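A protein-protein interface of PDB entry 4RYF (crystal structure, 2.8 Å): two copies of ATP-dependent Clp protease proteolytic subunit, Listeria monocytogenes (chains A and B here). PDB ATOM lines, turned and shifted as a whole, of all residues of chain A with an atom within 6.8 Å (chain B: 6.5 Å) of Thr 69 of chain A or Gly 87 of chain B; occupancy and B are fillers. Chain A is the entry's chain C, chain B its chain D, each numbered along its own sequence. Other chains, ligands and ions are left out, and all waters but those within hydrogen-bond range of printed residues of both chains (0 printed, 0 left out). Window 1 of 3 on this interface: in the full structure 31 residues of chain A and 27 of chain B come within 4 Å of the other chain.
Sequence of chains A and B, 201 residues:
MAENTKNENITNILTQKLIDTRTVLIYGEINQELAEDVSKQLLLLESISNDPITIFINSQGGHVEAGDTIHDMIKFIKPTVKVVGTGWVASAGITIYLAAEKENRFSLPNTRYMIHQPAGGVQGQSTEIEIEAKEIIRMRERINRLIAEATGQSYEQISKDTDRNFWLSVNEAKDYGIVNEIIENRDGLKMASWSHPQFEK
O of Ala 35 of chain A touches CE1 of Tyr 27 of chain B, 3.5 Å away. Tyr 27 of chain B touches Glu 36 of chain A (CD1 to N, 3.5 Å). Gly 87 of chain B touches Glu 65 of chain A (CA to O, 3.5 Å). Glu 65 of chain A touches Trp 88 of chain B. Asp 68 of chain A touches Asn 110 of chain B. Thr 69 of chain A touches Tyr 27 of chain B (CG2 to OH, 3.2 Å). OG1 of Thr 69 of chain A touches N of Gly 87 of chain B, 3.6 Å away. His 71 of chain A touches Asn 110 of chain B (CD2 to ND2, 3.5 Å). Leu 108 of chain B touches Asp 72 of chain A (CB to OD1, 3.3 Å). Met 73 of chain A touches Phe 56 of chain B.
Hydrophobic or aromatic side chains of chain A within 4 Å of the printed part of chain B: Ala 35, His 71 and Met 73. Of the 15 printed residues of chain B, 9 touch a printed residue of chain A. Hydrophobic or aromatic side chains of chain B that line the printed part of chain A: Tyr 27, Phe 56, Trp 88 and Leu 108. Among the printed residues, 17 pairs touch across the chains. Among the printed residues, Asp or Glu carboxylates within 4 Å of a Lys or Arg side-chain nitrogen of the other chain: Glu 65 of chain A with Arg 112 of chain B (2.8 Å).
N of Leu 108 of chain B is in hydrogen-bond range of O of Gly 85 of chain B, 2.9 Å away. The backbone NH of Val 89 of chain B lies within hydrogen-bond range of the backbone carbonyl oxygen of Arg 112 of chain B (3.1 Å). The backbone NH (N) of Ser 59 of chain B sits at hydrogen-bond distance from the backbone carbonyl oxygen (O) of Trp 88 of chain B (2.9 Å). The backbone carbonyl oxygen of Ile 57 of chain B lies within hydrogen-bond range of the backbone NH of Thr 86 of chain B (2.9 Å). The backbone carbonyl oxygen (O) of Glu 65 of chain A is in hydrogen-bond range of the side-chain hydroxyl (OG1) of Thr 69 of chain A, at 3.3 Å. The backbone NH (N) of Gly 87 of chain B is in hydrogen-bond range of the side-chain hydroxyl (OG1) of Thr 111 of chain B.
The side-chain carboxylate of Glu 65 of chain A is in salt-bridge range of the guanidinium group of Arg 112 of chain B. O of Glu 65 of chain A lies within hydrogen-bond range of ND2 of Asn 58 of chain B (3.1 Å). The side-chain hydroxyl of Thr 86 of chain B lies within hydrogen-bond range of the side-chain hydroxyl of Thr 69 of chain A (2.8 Å). OG of Ser 39 of chain A sits at hydrogen-bond distance from OH of Tyr 27 of chain B (2.9 Å). The side-chain amide oxygen (OD1) of Asn 110 of chain B sits at hydrogen-bond distance from the guanidinium group (NH2) of Arg 142 of chain A (2.9 Å). The side-chain hydroxyl of Thr 69 of chain A is in hydrogen-bond range of the side-chain amide nitrogen of Asn 58 of chain B, at 2.6 Å. OD1 of Asp 72 of chain A sits at hydrogen-bond distance from N of Asn 110 of chain B (2.9 Å).
Of chain B, only Tyr 27 (3.2 Å), Asn 58 (2.6 Å), Thr 86 (2.8 Å) and Gly 87 (3.6 Å) come within 4 Å of Thr 69 of chain A. Of the printed residues of chain A, Asn 58 of chain B touches Glu 65 and Thr 69. Of the printed residues of chain A, Phe 56 of chain B touches Met 73 (3.95 Å). Printed residues of chain B within 4 Å of Arg 142 of chain A: Asn 110 (2.9 Å). Printed residues of chain B within 4 Å of Ala 35 of chain A: Tyr 27 (3.5 Å). Printed residues of chain A within 4 Å of Trp 88 of chain B: Glu 65. Val 64 of chain A touches none of the printed residues of chain B. Gly 85 of chain B touches none of the printed residues of chain A. The nearest residue of chain A that does not touch Gly 87 of chain B is Asp 68 of chain A (4.1 Å).
No position is printed for both chains. Of the 17 pairs that touch across the chains among the printed residues, none has its exchanged pair printed and touching as well.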
ATOM      1  N   ALA A  35      -0.137   4.858  -6.544  1.00  0.00           N
ATOM      2  CA  ALA A  35       0.829   4.832  -5.451  1.00  0.00           C
ATOM      3  C   ALA A  35       1.265   3.409  -5.119  1.00  0.00           C
ATOM      4  O   ALA A  35       2.434   3.175  -4.818  1.00  0.00           O
ATOM      5  CB  ALA A  35       0.262   5.521  -4.220  1.00  0.00           C
ATOM      6  N   GLU A  36       0.327   2.464  -5.187  1.00  0.00           N
ATOM      7  CA  GLU A  36       0.632   1.055  -4.937  1.00  0.00           C
ATOM      8  C   GLU A  36       1.533   0.458  -6.023  1.00  0.00           C
ATOM      9  O   GLU A  36       2.483  -0.266  -5.710  1.00  0.00           O
ATOM     10  CB  GLU A  36      -0.650   0.230  -4.775  1.00  0.00           C
ATOM     11  CG  GLU A  36      -0.404  -1.177  -4.239  1.00  0.00           C
ATOM     12  CD  GLU A  36      -1.672  -1.992  -4.036  1.00  0.00           C
ATOM     13  OE1 GLU A  36      -2.786  -1.465  -4.249  1.00  0.00           O
ATOM     14  OE2 GLU A  36      -1.551  -3.176  -3.654  1.00  0.00           O
ATOM     15  N   SER A  39       5.037   2.102  -5.640  1.00  0.00           N
ATOM     16  CA  SER A  39       5.658   1.513  -4.450  1.00  0.00           C
ATOM     17  C   SER A  39       6.221   0.119  -4.730  1.00  0.00           C
ATOM     18  O   SER A  39       7.374  -0.162  -4.397  1.00  0.00           O
ATOM     19  CB  SER A  39       4.676   1.465  -3.278  1.00  0.00           C
ATOM     20  OG  SER A  39       4.431   2.762  -2.769  1.00  0.00           O
ATOM     21  N   LEU A  42       9.267   0.426  -7.172  1.00  0.00           N
ATOM     22  CA  LEU A  42      10.416   0.982  -6.457  1.00  0.00           C
ATOM     23  C   LEU A  42      11.038  -0.032  -5.497  1.00  0.00           C
ATOM     24  O   LEU A  42      12.260  -0.202  -5.482  1.00  0.00           O
ATOM     25  CB  LEU A  42      10.042   2.272  -5.717  1.00  0.00           C
ATOM     26  CG  LEU A  42       9.711   3.508  -6.559  1.00  0.00           C
ATOM     27  CD1 LEU A  42       9.380   4.686  -5.657  1.00  0.00           C
ATOM     28  CD2 LEU A  42      10.839   3.866  -7.519  1.00  0.00           C
ATOM     29  N   VAL A  64      -3.664  14.059  -2.825  1.00  0.00           N
ATOM     30  CA  VAL A  64      -2.435  14.547  -2.172  1.00  0.00           C
ATOM     31  C   VAL A  64      -1.737  13.501  -1.291  1.00  0.00           C
ATOM     32  O   VAL A  64      -0.507  13.407  -1.310  1.00  0.00           O
ATOM     33  CB  VAL A  64      -2.582  15.947  -1.483  1.00  0.00           C
ATOM     34  CG1 VAL A  64      -3.987  16.516  -1.611  1.00  0.00           C
ATOM     35  CG2 VAL A  64      -2.115  15.936  -0.030  1.00  0.00           C
ATOM     36  N   GLU A  65      -2.509  12.704  -0.553  1.00  0.00           N
ATOM     37  CA  GLU A  65      -1.932  11.663   0.304  1.00  0.00           C
ATOM     38  C   GLU A  65      -1.276  10.543  -0.492  1.00  0.00           C
ATOM     39  O   GLU A  65      -0.311   9.936  -0.031  1.00  0.00           O
ATOM     40  CB  GLU A  65      -2.971  11.089   1.264  1.00  0.00           C
ATOM     41  CG  GLU A  65      -3.223  11.960   2.485  1.00  0.00           C
ATOM     42  CD  GLU A  65      -4.196  13.098   2.223  1.00  0.00           C
ATOM     43  OE1 GLU A  65      -4.950  13.037   1.222  1.00  0.00           O
ATOM     44  OE2 GLU A  65      -4.212  14.053   3.031  1.00  0.00           O
ATOM     45  N   ALA A  66      -1.806  10.268  -1.681  1.00  0.00           N
ATOM     46  CA  ALA A  66      -1.180   9.322  -2.598  1.00  0.00           C
ATOM     47  C   ALA A  66       0.141   9.893  -3.108  1.00  0.00           C
ATOM     48  O   ALA A  66       1.129   9.169  -3.244  1.00  0.00           O
ATOM     49  CB  ALA A  66      -2.111   9.006  -3.756  1.00  0.00           C
ATOM     50  N   GLY A  67       0.146  11.198  -3.376  1.00  0.00           N
ATOM     51  CA  GLY A  67       1.347  11.913  -3.795  1.00  0.00           C
ATOM     52  C   GLY A  67       2.401  11.911  -2.706  1.00  0.00           C
ATOM     53  O   GLY A  67       3.589  11.745  -2.988  1.00  0.00           O
ATOM     54  N   ASP A  68       1.956  12.087  -1.461  1.00  0.00           N
ATOM     55  CA  ASP A  68       2.834  12.045  -0.291  1.00  0.00           C
ATOM     56  C   ASP A  68       3.547  10.705  -0.171  1.00  0.00           C
ATOM     57  O   ASP A  68       4.752  10.658   0.087  1.00  0.00           O
ATOM     58  CB  ASP A  68       2.042  12.327   0.991  1.00  0.00           C
ATOM     59  CG  ASP A  68       1.640  13.789   1.132  1.00  0.00           C
ATOM     60  OD1 ASP A  68       0.634  14.060   1.824  1.00  0.00           O
ATOM     61  OD2 ASP A  68       2.324  14.668   0.563  1.00  0.00           O
ATOM     62  N   THR A  69       2.797   9.620  -0.365  1.00  0.00           N
ATOM     63  CA  THR A  69       3.352   8.271  -0.285  1.00  0.00           C
ATOM     64  C   THR A  69       4.454   8.058  -1.317  1.00  0.00           C
ATOM     65  O   THR A  69       5.551   7.625  -0.969  1.00  0.00           O
ATOM     66  CB  THR A  69       2.255   7.191  -0.392  1.00  0.00           C
ATOM     67  OG1 THR A  69       1.437   7.239   0.782  1.00  0.00           O
ATOM     68  CG2 THR A  69       2.870   5.803  -0.500  1.00  0.00           C
ATOM     69  N   ILE A  70       4.169   8.388  -2.575  1.00  0.00           N
ATOM     70  CA  ILE A  70       5.163   8.266  -3.644  1.00  0.00           C
ATOM     71  C   ILE A  70       6.389   9.142  -3.360  1.00  0.00           C
ATOM     72  O   ILE A  70       7.525   8.695  -3.526  1.00  0.00           O
ATOM     73  CB  ILE A  70       4.562   8.572  -5.032  1.00  0.00           C
ATOM     74  CG1 ILE A  70       3.424   7.593  -5.341  1.00  0.00           C
ATOM     75  CG2 ILE A  70       5.632   8.487  -6.112  1.00  0.00           C
ATOM     76  CD1 ILE A  70       2.488   8.045  -6.442  1.00  0.00           C
ATOM     77  N   HIS A  71       6.152  10.376  -2.917  1.00  0.00           N
ATOM     78  CA  HIS A  71       7.226  11.285  -2.509  1.00  0.00           C
ATOM     79  C   HIS A  71       8.120  10.657  -1.439  1.00  0.00           C
ATOM     80  O   HIS A  71       9.342  10.605  -1.599  1.00  0.00           O
ATOM     81  CB  HIS A  71       6.648  12.613  -2.003  1.00  0.00           C
ATOM     82  CG  HIS A  71       7.635  13.464  -1.264  1.00  0.00           C
ATOM     83  ND1 HIS A  71       8.293  14.524  -1.850  1.00  0.00           N
ATOM     84  CD2 HIS A  71       8.075  13.410   0.016  1.00  0.00           C
ATOM     85  CE1 HIS A  71       9.096  15.086  -0.964  1.00  0.00           C
ATOM     86  NE2 HIS A  71       8.984  14.428   0.176  1.00  0.00           N
ATOM     87  N   ASP A  72       7.506  10.188  -0.353  1.00  0.00           N
ATOM     88  CA  ASP A  72       8.246   9.601   0.764  1.00  0.00           C
ATOM     89  C   ASP A  72       8.947   8.291   0.406  1.00  0.00           C
ATOM     90  O   ASP A  72      10.049   8.033   0.889  1.00  0.00           O
ATOM     91  CB  ASP A  72       7.339   9.421   1.987  1.00  0.00           C
ATOM     92  CG  ASP A  72       7.109  10.722   2.751  1.00  0.00           C
ATOM     93  OD1 ASP A  72       6.274  10.727   3.681  1.00  0.00           O
ATOM     94  OD2 ASP A  72       7.759  11.740   2.433  1.00  0.00           O
ATOM     95  N   MET A  73       8.315   7.480  -0.442  1.00  0.00           N
ATOM     96  CA  MET A  73       8.915   6.228  -0.918  1.00  0.00           C
ATOM     97  C   MET A  73      10.166   6.465  -1.762  1.00  0.00           C
ATOM     98  O   MET A  73      11.134   5.711  -1.659  1.00  0.00           O
ATOM     99  CB  MET A  73       7.902   5.392  -1.709  1.00  0.00           C
ATOM    100  CG  MET A  73       6.885   4.638  -0.858  1.00  0.00           C
ATOM    101  SD  MET A  73       7.572   3.372   0.232  1.00  0.00           S
ATOM    102  CE  MET A  73       8.521   2.380  -0.921  1.00  0.00           C
ATOM    103  N   ILE A  74      10.139   7.508  -2.593  1.00  0.00           N
ATOM    104  CA  ILE A  74      11.294   7.900  -3.407  1.00  0.00           C
ATOM    105  C   ILE A  74      12.508   8.209  -2.526  1.00  0.00           C
ATOM    106  O   ILE A  74      13.624   7.783  -2.826  1.00  0.00           O
ATOM    107  CB  ILE A  74      10.964   9.092  -4.336  1.00  0.00           C
ATOM    108  CG1 ILE A  74      10.128   8.619  -5.529  1.00  0.00           C
ATOM    109  CG2 ILE A  74      12.234   9.774  -4.835  1.00  0.00           C
ATOM    110  CD1 ILE A  74       9.358   9.721  -6.228  1.00  0.00           C
ATOM    111  N   ILE A  96       5.638  14.789  -5.921  1.00  0.00           N
ATOM    112  CA  ILE A  96       6.400  13.613  -6.349  1.00  0.00           C
ATOM    113  C   ILE A  96       7.703  14.029  -7.033  1.00  0.00           C
ATOM    114  O   ILE A  96       8.782  13.565  -6.656  1.00  0.00           O
ATOM    115  CB  ILE A  96       5.571  12.713  -7.292  1.00  0.00           C
ATOM    116  CG1 ILE A  96       4.381  12.111  -6.538  1.00  0.00           C
ATOM    117  CG2 ILE A  96       6.441  11.616  -7.901  1.00  0.00           C
ATOM    118  CD1 ILE A  96       3.287  11.573  -7.432  1.00  0.00           C
ATOM    119  N   ARG A 142       1.951  22.504   5.037  1.00  0.00           N
ATOM    120  CA  ARG A 142       2.893  21.391   4.882  1.00  0.00           C
ATOM    121  C   ARG A 142       3.438  21.316   3.454  1.00  0.00           C
ATOM    122  O   ARG A 142       4.655  21.238   3.255  1.00  0.00           O
ATOM    123  CB  ARG A 142       2.258  20.058   5.292  1.00  0.00           C
ATOM    124  CG  ARG A 142       3.218  18.875   5.244  1.00  0.00           C
ATOM    125  CD  ARG A 142       2.526  17.543   5.504  1.00  0.00           C
ATOM    126  NE  ARG A 142       1.386  17.296   4.614  1.00  0.00           N
ATOM    127  CZ  ARG A 142       1.474  16.869   3.355  1.00  0.00           C
ATOM    128  NH1 ARG A 142       0.370  16.678   2.647  1.00  0.00           N
ATOM    129  NH2 ARG A 142       2.655  16.637   2.794  1.00  0.00           N
ATOM    130  N   TYR B  27      -3.137   0.008   0.683  1.00  0.00           N
ATOM    131  CA  TYR B  27      -3.421   1.319   0.103  1.00  0.00           C
ATOM    132  C   TYR B  27      -4.888   1.407  -0.292  1.00  0.00           C
ATOM    133  O   TYR B  27      -5.394   0.551  -1.020  1.00  0.00           O
ATOM    134  CB  TYR B  27      -2.554   1.557  -1.140  1.00  0.00           C
ATOM    135  CG  TYR B  27      -1.083   1.847  -0.898  1.00  0.00           C
ATOM    136  CD1 TYR B  27      -0.360   2.631  -1.796  1.00  0.00           C
ATOM    137  CD2 TYR B  27      -0.410   1.338   0.215  1.00  0.00           C
ATOM    138  CE1 TYR B  27       0.986   2.896  -1.598  1.00  0.00           C
ATOM    139  CE2 TYR B  27       0.934   1.601   0.425  1.00  0.00           C
ATOM    140  CZ  TYR B  27       1.627   2.379  -0.484  1.00  0.00           C
ATOM    141  OH  TYR B  27       2.960   2.638  -0.277  1.00  0.00           O
ATOM    142  N   PHE B  56       3.127  -1.258   4.793  1.00  0.00           N
ATOM    143  CA  PHE B  56       2.937   0.160   4.512  1.00  0.00           C
ATOM    144  C   PHE B  56       1.444   0.447   4.403  1.00  0.00           C
ATOM    145  O   PHE B  56       0.746  -0.174   3.596  1.00  0.00           O
ATOM    146  CB  PHE B  56       3.657   0.563   3.223  1.00  0.00           C
ATOM    147  CG  PHE B  56       5.157   0.528   3.326  1.00  0.00           C
ATOM    148  CD1 PHE B  56       5.861  -0.646   3.063  1.00  0.00           C
ATOM    149  CD2 PHE B  56       5.872   1.670   3.676  1.00  0.00           C
ATOM    150  CE1 PHE B  56       7.245  -0.682   3.156  1.00  0.00           C
ATOM    151  CE2 PHE B  56       7.256   1.639   3.773  1.00  0.00           C
ATOM    152  CZ  PHE B  56       7.943   0.463   3.512  1.00  0.00           C
ATOM    153  N   ILE B  57       0.957   1.375   5.225  1.00  0.00           N
ATOM    154  CA  ILE B  57      -0.467   1.721   5.236  1.00  0.00           C
ATOM    155  C   ILE B  57      -0.726   3.146   4.759  1.00  0.00           C
ATOM    156  O   ILE B  57      -0.235   4.116   5.346  1.00  0.00           O
ATOM    157  CB  ILE B  57      -1.118   1.532   6.626  1.00  0.00           C
ATOM    158  CG1 ILE B  57      -0.573   0.283   7.321  1.00  0.00           C
ATOM    159  CG2 ILE B  57      -2.638   1.466   6.496  1.00  0.00           C
ATOM    160  CD1 ILE B  57      -1.032   0.114   8.754  1.00  0.00           C
ATOM    161  N   ASN B  58      -1.492   3.249   3.677  1.00  0.00           N
ATOM    162  CA  ASN B  58      -2.075   4.504   3.231  1.00  0.00           C
ATOM    163  C   ASN B  58      -3.569   4.263   3.087  1.00  0.00           C
ATOM    164  O   ASN B  58      -4.031   3.781   2.050  1.00  0.00           O
ATOM    165  CB  ASN B  58      -1.464   4.952   1.895  1.00  0.00           C
ATOM    166  CG  ASN B  58      -2.021   6.281   1.401  1.00  0.00           C
ATOM    167  OD1 ASN B  58      -3.178   6.619   1.638  1.00  0.00           O
ATOM    168  ND2 ASN B  58      -1.194   7.035   0.689  1.00  0.00           N
ATOM    169  N   SER B  59      -4.326   4.581   4.132  1.00  0.00           N
ATOM    170  CA  SER B  59      -5.754   4.284   4.135  1.00  0.00           C
ATOM    171  C   SER B  59      -6.599   5.303   4.883  1.00  0.00           C
ATOM    172  O   SER B  59      -6.284   5.692   6.009  1.00  0.00           O
ATOM    173  CB  SER B  59      -6.008   2.886   4.704  1.00  0.00           C
ATOM    174  OG  SER B  59      -7.396   2.602   4.727  1.00  0.00           O
ATOM    175  N   GLY B  85       3.239   4.002   8.550  1.00  0.00           N
ATOM    176  CA  GLY B  85       2.168   4.891   8.110  1.00  0.00           C
ATOM    177  C   GLY B  85       2.670   5.826   7.030  1.00  0.00           C
ATOM    178  O   GLY B  85       3.742   6.420   7.169  1.00  0.00           O
ATOM    179  N   THR B  86       1.906   5.947   5.948  1.00  0.00           N
ATOM    180  CA  THR B  86       2.276   6.826   4.841  1.00  0.00           C
ATOM    181  C   THR B  86       1.056   7.507   4.212  1.00  0.00           C
ATOM    182  O   THR B  86       0.039   6.862   3.959  1.00  0.00           O
ATOM    183  CB  THR B  86       3.138   6.091   3.782  1.00  0.00           C
ATOM    184  OG1 THR B  86       3.422   6.973   2.690  1.00  0.00           O
ATOM    185  CG2 THR B  86       2.451   4.826   3.261  1.00  0.00           C
ATOM    186  N   GLY B  87       1.163   8.813   3.978  1.00  0.00           N
ATOM    187  CA  GLY B  87       0.067   9.597   3.404  1.00  0.00           C
ATOM    188  C   GLY B  87      -0.966   9.953   4.454  1.00  0.00           C
ATOM    189  O   GLY B  87      -0.924  11.037   5.037  1.00  0.00           O
ATOM    190  N   TRP B  88      -1.912   9.045   4.678  1.00  0.00           N
ATOM    191  CA  TRP B  88      -2.796   9.128   5.839  1.00  0.00           C
ATOM    192  C   TRP B  88      -3.170   7.756   6.374  1.00  0.00           C
ATOM    193  O   TRP B  88      -3.129   6.761   5.651  1.00  0.00           O
ATOM    194  CB  TRP B  88      -4.054   9.983   5.579  1.00  0.00           C
ATOM    195  CG  TRP B  88      -4.905   9.599   4.385  1.00  0.00           C
ATOM    196  CD1 TRP B  88      -4.747   8.517   3.562  1.00  0.00           C
ATOM    197  CD2 TRP B  88      -6.066  10.297   3.908  1.00  0.00           C
ATOM    198  NE1 TRP B  88      -5.723   8.511   2.596  1.00  0.00           N
ATOM    199  CE2 TRP B  88      -6.547   9.588   2.785  1.00  0.00           C
ATOM    200  CE3 TRP B  88      -6.739  11.458   4.316  1.00  0.00           C
ATOM    201  CZ2 TRP B  88      -7.676   9.997   2.067  1.00  0.00           C
ATOM    202  CZ3 TRP B  88      -7.862  11.865   3.600  1.00  0.00           C
ATOM    203  CH2 TRP B  88      -8.316  11.135   2.487  1.00  0.00           C
ATOM    204  N   VAL B  89      -3.498   7.720   7.661  1.00  0.00           N
ATOM    205  CA  VAL B  89      -4.005   6.526   8.323  1.00  0.00           C
ATOM    206  C   VAL B  89      -5.199   6.985   9.153  1.00  0.00           C
ATOM    207  O   VAL B  89      -5.037   7.746  10.110  1.00  0.00           O
ATOM    208  CB  VAL B  89      -2.936   5.865   9.225  1.00  0.00           C
ATOM    209  CG1 VAL B  89      -3.468   4.581   9.841  1.00  0.00           C
ATOM    210  CG2 VAL B  89      -1.664   5.571   8.443  1.00  0.00           C
ATOM    211  N   LEU B 108       6.290   7.624   7.905  1.00  0.00           N
ATOM    212  CA  LEU B 108       7.008   8.488   6.980  1.00  0.00           C
ATOM    213  C   LEU B 108       6.613   9.942   7.279  1.00  0.00           C
ATOM    214  O   LEU B 108       5.544  10.181   7.848  1.00  0.00           O
ATOM    215  CB  LEU B 108       6.691   8.081   5.538  1.00  0.00           C
ATOM    216  CG  LEU B 108       7.586   7.043   4.836  1.00  0.00           C
ATOM    217  CD1 LEU B 108       8.339   6.123   5.784  1.00  0.00           C
ATOM    218  CD2 LEU B 108       6.774   6.232   3.841  1.00  0.00           C
ATOM    219  N   ASN B 110       5.525  12.729   5.714  1.00  0.00           N
ATOM    220  CA  ASN B 110       4.292  13.333   5.211  1.00  0.00           C
ATOM    221  C   ASN B 110       3.071  12.432   5.392  1.00  0.00           C
ATOM    222  O   ASN B 110       2.503  11.913   4.424  1.00  0.00           O
ATOM    223  CB  ASN B 110       4.453  13.750   3.750  1.00  0.00           C
ATOM    224  CG  ASN B 110       5.490  14.835   3.573  1.00  0.00           C
ATOM    225  OD1 ASN B 110       5.242  16.004   3.873  1.00  0.00           O
ATOM    226  ND2 ASN B 110       6.661  14.455   3.080  1.00  0.00           N
ATOM    227  N   THR B 111       2.684  12.248   6.650  1.00  0.00           N
ATOM    228  CA  THR B 111       1.530  11.434   6.993  1.00  0.00           C
ATOM    229  C   THR B 111       0.705  12.166   8.036  1.00  0.00           C
ATOM    230  O   THR B 111       1.256  12.795   8.938  1.00  0.00           O
ATOM    231  CB  THR B 111       1.954  10.056   7.541  1.00  0.00           C
ATOM    232  OG1 THR B 111       2.975   9.502   6.704  1.00  0.00           O
ATOM    233  CG2 THR B 111       0.768   9.094   7.591  1.00  0.00           C
ATOM    234  N   ARG B 112      -0.614  12.102   7.894  1.00  0.00           N
ATOM    235  CA  ARG B 112      -1.505  12.572   8.943  1.00  0.00           C
ATOM    236  C   ARG B 112      -2.403  11.443   9.433  1.00  0.00           C
ATOM    237  O   ARG B 112      -2.625  10.456   8.727  1.00  0.00           O
ATOM    238  CB  ARG B 112      -2.300  13.809   8.510  1.00  0.00           C
ATOM    239  CG  ARG B 112      -3.269  13.603   7.360  1.00  0.00           C
ATOM    240  CD  ARG B 112      -3.746  14.944   6.833  1.00  0.00           C
ATOM    241  NE  ARG B 112      -4.618  14.786   5.673  1.00  0.00           N
ATOM    242  CZ  ARG B 112      -5.882  15.199   5.613  1.00  0.00           C
ATOM    243  NH1 ARG B 112      -6.586  14.998   4.510  1.00  0.00           N
ATOM    244  NH2 ARG B 112      -6.441  15.823   6.639  1.00  0.00           N
ATOM    245  N   TYR B 113      -2.893  11.592  10.657  1.00  0.00           N
ATOM    246  CA  TYR B 113      -3.605  10.527  11.345  1.00  0.00           C
ATOM    247  C   TYR B 113      -4.944  11.030  11.840  1.00  0.00           C
ATOM    248  O   TYR B 113      -5.073  12.195  12.215  1.00  0.00           O
ATOM    249  CB  TYR B 113      -2.755  10.003  12.508  1.00  0.00           C
ATOM    250  CG  TYR B 113      -1.525   9.266  12.037  1.00  0.00           C
ATOM    251  CD1 TYR B 113      -1.503   7.877  11.998  1.00  0.00           C
ATOM    252  CD2 TYR B 113      -0.391   9.957  11.602  1.00  0.00           C
ATOM    253  CE1 TYR B 113      -0.385   7.192  11.551  1.00  0.00           C
ATOM    254  CE2 TYR B 113       0.732   9.283  11.153  1.00  0.00           C
ATOM    255  CZ  TYR B 113       0.726   7.900  11.128  1.00  0.00           C
ATOM    256  OH  TYR B 113       1.828   7.213  10.687  1.00  0.00           O
